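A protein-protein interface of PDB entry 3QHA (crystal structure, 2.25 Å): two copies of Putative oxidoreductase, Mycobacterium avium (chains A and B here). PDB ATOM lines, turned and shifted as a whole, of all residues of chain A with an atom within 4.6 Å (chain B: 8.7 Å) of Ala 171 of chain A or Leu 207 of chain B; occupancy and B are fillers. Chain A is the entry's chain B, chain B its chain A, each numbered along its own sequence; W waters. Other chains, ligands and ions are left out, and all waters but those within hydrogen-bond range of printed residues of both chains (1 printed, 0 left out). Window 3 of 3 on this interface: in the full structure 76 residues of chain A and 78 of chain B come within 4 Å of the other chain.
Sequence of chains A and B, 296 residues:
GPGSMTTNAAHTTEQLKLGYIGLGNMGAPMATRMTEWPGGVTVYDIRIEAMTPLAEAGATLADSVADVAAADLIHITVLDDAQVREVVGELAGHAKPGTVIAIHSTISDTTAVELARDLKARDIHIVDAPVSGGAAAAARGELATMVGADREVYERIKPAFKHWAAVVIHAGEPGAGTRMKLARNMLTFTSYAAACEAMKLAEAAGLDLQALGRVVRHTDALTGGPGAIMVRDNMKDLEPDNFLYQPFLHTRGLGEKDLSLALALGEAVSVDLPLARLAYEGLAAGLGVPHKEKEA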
ATOM      1  N   VAL A 147       3.726 -22.398  23.600  1.00  0.00           N
ATOM      2  CA  VAL A 147       4.351 -21.869  22.396  1.00  0.00           C
ATOM      3  C   VAL A 147       3.437 -21.966  21.175  1.00  0.00           C
ATOM      4  O   VAL A 147       3.006 -23.057  20.803  1.00  0.00           O
ATOM      5  CB  VAL A 147       5.658 -22.633  22.109  1.00  0.00           C
ATOM      6  CG1 VAL A 147       6.364 -22.069  20.888  1.00  0.00           C
ATOM      7  CG2 VAL A 147       6.571 -22.588  23.330  1.00  0.00           C
ATOM      8  N   ILE A 169       5.102 -26.585  25.985  1.00  0.00           N
ATOM      9  CA  ILE A 169       3.901 -26.984  25.268  1.00  0.00           C
ATOM     10  C   ILE A 169       3.889 -26.348  23.885  1.00  0.00           C
ATOM     11  O   ILE A 169       4.103 -25.139  23.748  1.00  0.00           O
ATOM     12  CB  ILE A 169       2.612 -26.541  26.004  1.00  0.00           C
ATOM     13  CG1 ILE A 169       2.586 -27.064  27.445  1.00  0.00           C
ATOM     14  CG2 ILE A 169       1.379 -27.012  25.249  1.00  0.00           C
ATOM     15  CD1 ILE A 169       2.654 -28.580  27.568  1.00  0.00           C
ATOM     16  N   HIS A 170       3.643 -27.170  22.868  1.00  0.00           N
ATOM     17  CA  HIS A 170       3.352 -26.672  21.533  1.00  0.00           C
ATOM     18  C   HIS A 170       1.842 -26.514  21.439  1.00  0.00           C
ATOM     19  O   HIS A 170       1.116 -27.459  21.113  1.00  0.00           O
ATOM     20  CB  HIS A 170       3.880 -27.619  20.454  1.00  0.00           C
ATOM     21  CG  HIS A 170       3.793 -27.055  19.070  1.00  0.00           C
ATOM     22  ND1 HIS A 170       3.756 -27.845  17.943  1.00  0.00           N
ATOM     23  CD2 HIS A 170       3.713 -25.775  18.635  1.00  0.00           C
ATOM     24  CE1 HIS A 170       3.670 -27.077  16.873  1.00  0.00           C
ATOM     25  NE2 HIS A 170       3.641 -25.816  17.265  1.00  0.00           N
ATOM     26  N   ALA A 171       1.379 -25.308  21.754  1.00  0.00           N
ATOM     27  CA  ALA A 171      -0.049 -25.028  21.882  1.00  0.00           C
ATOM     28  C   ALA A 171      -0.741 -25.026  20.525  1.00  0.00           C
ATOM     29  O   ALA A 171      -1.940 -25.278  20.440  1.00  0.00           O
ATOM     30  CB  ALA A 171      -0.261 -23.698  22.582  1.00  0.00           C
ATOM     31  N   GLY A 172       0.024 -24.736  19.476  1.00  0.00           N
ATOM     32  CA  GLY A 172      -0.498 -24.675  18.115  1.00  0.00           C
ATOM     33  C   GLY A 172       0.304 -23.724  17.245  1.00  0.00           C
ATOM     34  O   GLY A 172       1.502 -23.533  17.456  1.00  0.00           O
ATOM     35  N   ALA A 176      -1.622 -19.304  19.390  1.00  0.00           N
ATOM     36  CA  ALA A 176      -2.121 -20.367  20.270  1.00  0.00           C
ATOM     37  C   ALA A 176      -1.474 -20.337  21.654  1.00  0.00           C
ATOM     38  O   ALA A 176      -2.112 -20.677  22.649  1.00  0.00           O
ATOM     39  CB  ALA A 176      -1.906 -21.733  19.625  1.00  0.00           C
ATOM     40  N   GLY A 177      -0.204 -19.946  21.708  1.00  0.00           N
ATOM     41  CA  GLY A 177       0.488 -19.778  22.976  1.00  0.00           C
ATOM     42  C   GLY A 177      -0.207 -18.734  23.826  1.00  0.00           C
ATOM     43  O   GLY A 177      -0.522 -18.981  24.991  1.00  0.00           O
ATOM     44  N   ARG A 179      -3.240 -17.629  23.654  1.00  0.00           N
ATOM     45  CA  ARG A 179      -4.570 -18.078  24.049  1.00  0.00           C
ATOM     46  C   ARG A 179      -4.556 -19.116  25.177  1.00  0.00           C
ATOM     47  O   ARG A 179      -5.429 -19.078  26.045  1.00  0.00           O
ATOM     48  CB  ARG A 179      -5.346 -18.589  22.834  1.00  0.00           C
ATOM     49  CG  ARG A 179      -5.730 -17.472  21.861  1.00  0.00           C
ATOM     50  CD  ARG A 179      -6.718 -17.939  20.807  1.00  0.00           C
ATOM     51  NE  ARG A 179      -6.135 -18.946  19.923  1.00  0.00           N
ATOM     52  CZ  ARG A 179      -5.422 -18.691  18.822  1.00  0.00           C
ATOM     53  NH1 ARG A 179      -5.175 -17.441  18.428  1.00  0.00           N
ATOM     54  NH2 ARG A 179      -4.943 -19.703  18.104  1.00  0.00           N
ATOM     55  N   MET A 180      -3.581 -20.026  25.188  1.00  0.00           N
ATOM     56  CA  MET A 180      -3.443 -20.946  26.324  1.00  0.00           C
ATOM     57  C   MET A 180      -3.079 -20.154  27.582  1.00  0.00           C
ATOM     58  O   MET A 180      -3.572 -20.452  28.669  1.00  0.00           O
ATOM     59  CB  MET A 180      -2.404 -22.046  26.067  1.00  0.00           C
ATOM     60  CG  MET A 180      -2.445 -23.166  27.115  1.00  0.00           C
ATOM     61  SD  MET A 180      -1.463 -24.631  26.722  1.00  0.00           S
ATOM     62  CE  MET A 180      -2.419 -25.333  25.380  1.00  0.00           C
ATOM     63  N   ALA B 198     -12.041 -22.228  32.764  1.00  0.00           N
ATOM     64  CA  ALA B 198     -10.824 -22.084  31.952  1.00  0.00           C
ATOM     65  C   ALA B 198     -10.742 -23.154  30.858  1.00  0.00           C
ATOM     66  O   ALA B 198     -10.293 -22.878  29.740  1.00  0.00           O
ATOM     67  CB  ALA B 198      -9.582 -22.130  32.835  1.00  0.00           C
ATOM     68  N   MET B 199     -11.189 -24.365  31.190  1.00  0.00           N
ATOM     69  CA  MET B 199     -11.189 -25.492  30.256  1.00  0.00           C
ATOM     70  C   MET B 199     -12.210 -25.298  29.130  1.00  0.00           C
ATOM     71  O   MET B 199     -11.945 -25.653  27.979  1.00  0.00           O
ATOM     72  CB  MET B 199     -11.480 -26.805  31.000  1.00  0.00           C
ATOM     73  CG  MET B 199     -10.392 -27.231  31.982  1.00  0.00           C
ATOM     74  SD  MET B 199     -10.928 -28.498  33.159  1.00  0.00           S
ATOM     75  CE  MET B 199     -11.104 -29.926  32.094  1.00  0.00           C
ATOM     76  N   LYS B 200     -13.376 -24.748  29.462  1.00  0.00           N
ATOM     77  CA  LYS B 200     -14.393 -24.452  28.455  1.00  0.00           C
ATOM     78  C   LYS B 200     -13.861 -23.429  27.453  1.00  0.00           C
ATOM     79  O   LYS B 200     -14.080 -23.564  26.249  1.00  0.00           O
ATOM     80  CB  LYS B 200     -15.682 -23.938  29.106  1.00  0.00           C
ATOM     81  N   LEU B 201     -13.150 -22.418  27.952  1.00  0.00           N
ATOM     82  CA  LEU B 201     -12.563 -21.388  27.092  1.00  0.00           C
ATOM     83  C   LEU B 201     -11.462 -21.966  26.202  1.00  0.00           C
ATOM     84  O   LEU B 201     -11.435 -21.715  24.996  1.00  0.00           O
ATOM     85  CB  LEU B 201     -12.002 -20.237  27.930  1.00  0.00           C
ATOM     86  CG  LEU B 201     -11.344 -19.097  27.144  1.00  0.00           C
ATOM     87  CD1 LEU B 201     -12.366 -18.416  26.237  1.00  0.00           C
ATOM     88  CD2 LEU B 201     -10.701 -18.097  28.085  1.00  0.00           C
ATOM     89  N   ALA B 202     -10.556 -22.728  26.811  1.00  0.00           N
ATOM     90  CA  ALA B 202      -9.482 -23.405  26.086  1.00  0.00           C
ATOM     91  C   ALA B 202     -10.020 -24.267  24.939  1.00  0.00           C
ATOM     92  O   ALA B 202      -9.495 -24.224  23.829  1.00  0.00           O
ATOM     93  CB  ALA B 202      -8.667 -24.257  27.042  1.00  0.00           C
ATOM     94  N   GLU B 203     -11.074 -25.034  25.215  1.00  0.00           N
ATOM     95  CA  GLU B 203     -11.669 -25.938  24.225  1.00  0.00           C
ATOM     96  C   GLU B 203     -12.280 -25.173  23.051  1.00  0.00           C
ATOM     97  O   GLU B 203     -12.098 -25.552  21.892  1.00  0.00           O
ATOM     98  CB  GLU B 203     -12.724 -26.831  24.885  1.00  0.00           C
ATOM     99  CG  GLU B 203     -13.525 -27.701  23.924  1.00  0.00           C
ATOM    100  CD  GLU B 203     -14.415 -28.686  24.650  1.00  0.00           C
ATOM    101  OE1 GLU B 203     -13.911 -29.742  25.078  1.00  0.00           O
ATOM    102  OE2 GLU B 203     -15.622 -28.408  24.790  1.00  0.00           O
ATOM    103  N   ALA B 204     -12.998 -24.097  23.357  1.00  0.00           N
ATOM    104  CA  ALA B 204     -13.564 -23.226  22.328  1.00  0.00           C
ATOM    105  C   ALA B 204     -12.465 -22.543  21.503  1.00  0.00           C
ATOM    106  O   ALA B 204     -12.698 -22.143  20.364  1.00  0.00           O
ATOM    107  CB  ALA B 204     -14.476 -22.183  22.962  1.00  0.00           C
ATOM    108  N   ALA B 205     -11.275 -22.414  22.087  1.00  0.00           N
ATOM    109  CA  ALA B 205     -10.114 -21.870  21.386  1.00  0.00           C
ATOM    110  C   ALA B 205      -9.327 -22.947  20.628  1.00  0.00           C
ATOM    111  O   ALA B 205      -8.311 -22.645  20.008  1.00  0.00           O
ATOM    112  CB  ALA B 205      -9.201 -21.149  22.368  1.00  0.00           C
ATOM    113  N   GLY B 206      -9.785 -24.196  20.680  1.00  0.00           N
ATOM    114  CA  GLY B 206      -9.156 -25.283  19.932  1.00  0.00           C
ATOM    115  C   GLY B 206      -7.879 -25.817  20.561  1.00  0.00           C
ATOM    116  O   GLY B 206      -7.037 -26.387  19.866  1.00  0.00           O
ATOM    117  N   LEU B 207      -7.745 -25.653  21.876  1.00  0.00           N
ATOM    118  CA  LEU B 207      -6.514 -26.004  22.589  1.00  0.00           C
ATOM    119  C   LEU B 207      -6.589 -27.375  23.267  1.00  0.00           C
ATOM    120  O   LEU B 207      -7.674 -27.908  23.508  1.00  0.00           O
ATOM    121  CB  LEU B 207      -6.193 -24.933  23.636  1.00  0.00           C
ATOM    122  CG  LEU B 207      -5.940 -23.519  23.105  1.00  0.00           C
ATOM    123  CD1 LEU B 207      -5.871 -22.519  24.251  1.00  0.00           C
ATOM    124  CD2 LEU B 207      -4.665 -23.463  22.270  1.00  0.00           C
ATOM    125  N   ASP B 208      -5.418 -27.933  23.566  1.00  0.00           N
ATOM    126  CA  ASP B 208      -5.308 -29.194  24.296  1.00  0.00           C
ATOM    127  C   ASP B 208      -5.511 -28.916  25.790  1.00  0.00           C
ATOM    128  O   ASP B 208      -4.686 -28.256  26.418  1.00  0.00           O
ATOM    129  CB  ASP B 208      -3.931 -29.821  24.032  1.00  0.00           C
ATOM    130  CG  ASP B 208      -3.715 -31.136  24.769  1.00  0.00           C
ATOM    131  OD1 ASP B 208      -4.391 -31.395  25.790  1.00  0.00           O
ATOM    132  OD2 ASP B 208      -2.840 -31.910  24.329  1.00  0.00           O
ATOM    133  N   LEU B 209      -6.607 -29.430  26.351  1.00  0.00           N
ATOM    134  CA  LEU B 209      -6.964 -29.165  27.751  1.00  0.00           C
ATOM    135  C   LEU B 209      -6.032 -29.871  28.734  1.00  0.00           C
ATOM    136  O   LEU B 209      -5.764 -29.360  29.825  1.00  0.00           O
ATOM    137  CB  LEU B 209      -8.410 -29.586  28.035  1.00  0.00           C
ATOM    138  CG  LEU B 209      -9.488 -29.036  27.092  1.00  0.00           C
ATOM    139  CD1 LEU B 209     -10.873 -29.449  27.564  1.00  0.00           C
ATOM    140  CD2 LEU B 209      -9.386 -27.521  26.970  1.00  0.00           C
ATOM    141  N   GLN B 210      -5.548 -31.048  28.344  1.00  0.00           N
ATOM    142  CA  GLN B 210      -4.648 -31.828  29.189  1.00  0.00           C
ATOM    143  C   GLN B 210      -3.285 -31.148  29.299  1.00  0.00           C
ATOM    144  O   GLN B 210      -2.635 -31.223  30.341  1.00  0.00           O
ATOM    145  CB  GLN B 210      -4.487 -33.247  28.636  1.00  0.00           C
ATOM    146  CG  GLN B 210      -5.781 -34.064  28.598  1.00  0.00           C
ATOM    147  CD  GLN B 210      -6.194 -34.609  29.956  1.00  0.00           C
ATOM    148  OE1 GLN B 210      -5.666 -34.206  30.995  1.00  0.00           O
ATOM    149  NE2 GLN B 210      -7.146 -35.536  29.951  1.00  0.00           N
ATOM    150  N   ALA B 211      -2.859 -30.490  28.222  1.00  0.00           N
ATOM    151  CA  ALA B 211      -1.617 -29.722  28.224  1.00  0.00           C
ATOM    152  C   ALA B 211      -1.760 -28.508  29.136  1.00  0.00           C
ATOM    153  O   ALA B 211      -0.856 -28.208  29.922  1.00  0.00           O
ATOM    154  CB  ALA B 211      -1.248 -29.287  26.811  1.00  0.00           C
ATOM    155  N   LEU B 212      -2.897 -27.815  29.029  1.00  0.00           N
ATOM    156  CA  LEU B 212      -3.204 -26.690  29.917  1.00  0.00           C
ATOM    157  C   LEU B 212      -3.135 -27.143  31.371  1.00  0.00           C
ATOM    158  O   LEU B 212      -2.488 -26.498  32.197  1.00  0.00           O
ATOM    159  CB  LEU B 212      -4.589 -26.111  29.610  1.00  0.00           C
ATOM    160  CG  LEU B 212      -5.123 -25.002  30.528  1.00  0.00           C
ATOM    161  CD1 LEU B 212      -4.227 -23.774  30.502  1.00  0.00           C
ATOM    162  CD2 LEU B 212      -6.541 -24.632  30.133  1.00  0.00           C
ATOM    163  N   VAL B 215       0.365 -27.464  32.594  1.00  0.00           N
ATOM    164  CA  VAL B 215       0.973 -26.153  32.849  1.00  0.00           C
ATOM    165  C   VAL B 215       0.524 -25.607  34.206  1.00  0.00           C
ATOM    166  O   VAL B 215       1.348 -25.163  35.006  1.00  0.00           O
ATOM    167  CB  VAL B 215       0.642 -25.133  31.727  1.00  0.00           C
ATOM    168  CG1 VAL B 215       1.088 -23.733  32.116  1.00  0.00           C
ATOM    169  CG2 VAL B 215       1.297 -25.553  30.419  1.00  0.00           C
ATOM    170  N   LEU B 265     -11.388 -12.774  24.606  1.00  0.00           N
ATOM    171  CA  LEU B 265     -11.286 -14.070  23.930  1.00  0.00           C
ATOM    172  C   LEU B 265     -12.597 -14.837  24.063  1.00  0.00           C
ATOM    173  O   LEU B 265     -13.098 -15.387  23.083  1.00  0.00           O
ATOM    174  CB  LEU B 265     -10.137 -14.913  24.498  1.00  0.00           C
ATOM    175  CG  LEU B 265      -9.880 -16.266  23.819  1.00  0.00           C
ATOM    176  CD1 LEU B 265      -9.566 -16.091  22.333  1.00  0.00           C
ATOM    177  CD2 LEU B 265      -8.754 -17.008  24.518  1.00  0.00           C
HETATM  178  O   HOH W   1      -3.116 -26.716  22.408  1.00  0.00           O
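Of the printed residues of chain B, Ile 169 of chain A touches Ala 211 (3.8 Å) and Val 215 (3.6 Å). His 170 of chain A touches none of the printed residues of chain B. Ala 171 of chain A touches one residue of chain B. Of the printed residues of chain B, Arg 179 of chain A touches Leu 207 (3.8 Å) and Leu 265 (3.7 Å). Lys 200 of chain B touches none of the printed residues of chain A. Leu 207 of chain B touches four residues of chain A. Of the printed residues of chain A, Asp 208 of chain B touches Met 180 (3.8 Å). Of the printed residues of chain A, Val 215 of chain B touches Ile 169. The nearest printed residue of chain A that does not touch Leu 207 of chain B is Gly 172 of chain A (5.6 Å). The nearest printed residue of chain B that does not touch Ile 169 of chain A is Leu 212 of chain B (5.8 Å).
O of Ala 202 of chain B lies within hydrogen-bond range of N of Leu 207 of chain B, 3.0 Å away. OD1 of Asp 208 of chain B lies within hydrogen-bond range of N of Gln 210 of chain B, at 2.8 Å. The side-chain carboxylate (OD1) of Asp 208 of chain B is in hydrogen-bond range of the backbone NH (N) of Ala 211 of chain B. N of Val 147 of chain A lies within hydrogen-bond range of O of Ile 169 of chain A, 2.8 Å away. The backbone NH (N) of Ala 171 of chain A sits at hydrogen-bond distance from the backbone carbonyl oxygen (O) of Val 147 of chain A.
Water W1 bridges the backbone carbonyl oxygen of Ala 171 of chain A and the backbone NH of Asp 208 of chain B.
Among the printed residues, merely in contact across the chains: Ile 169 of chain A with Ala 211 of chain B (3.8 Å), Ile 169 of chain A with Val 215 of chain B (3.6 Å), Ala 171 of chain A with Leu 207 of chain B (3.8 Å), Ala 176 of chain A with Leu 207 of chain B (3.8 Å), Arg 179 of chain A with Leu 207 of chain B (3.8 Å), Arg 179 of chain A with Leu 265 of chain B (3.7 Å), Met 180 of chain A with Leu 207 of chain B (3.5 Å), Met 180 of chain A with Asp 208 of chain B (3.8 Å) and Met 180 of chain A with Leu 212 of chain B (3.9 Å).
No position is printed for both chains.
Printed residues of chain A that touch a printed residue of chain B: Ile 169, Ala 171, Ala 176, Arg 179 and Met 180. Hydrophobic or aromatic side chains of chain A within 4 Å of the printed part of chain B: Ile 169 and Met 180. Of the 17 printed residues of chain B, 6 touch a printed residue of chain A. Among the printed residues, no Asp or Glu carboxylate lies within 4 Å of a Lys or Arg side-chain nitrogen of the other chain.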
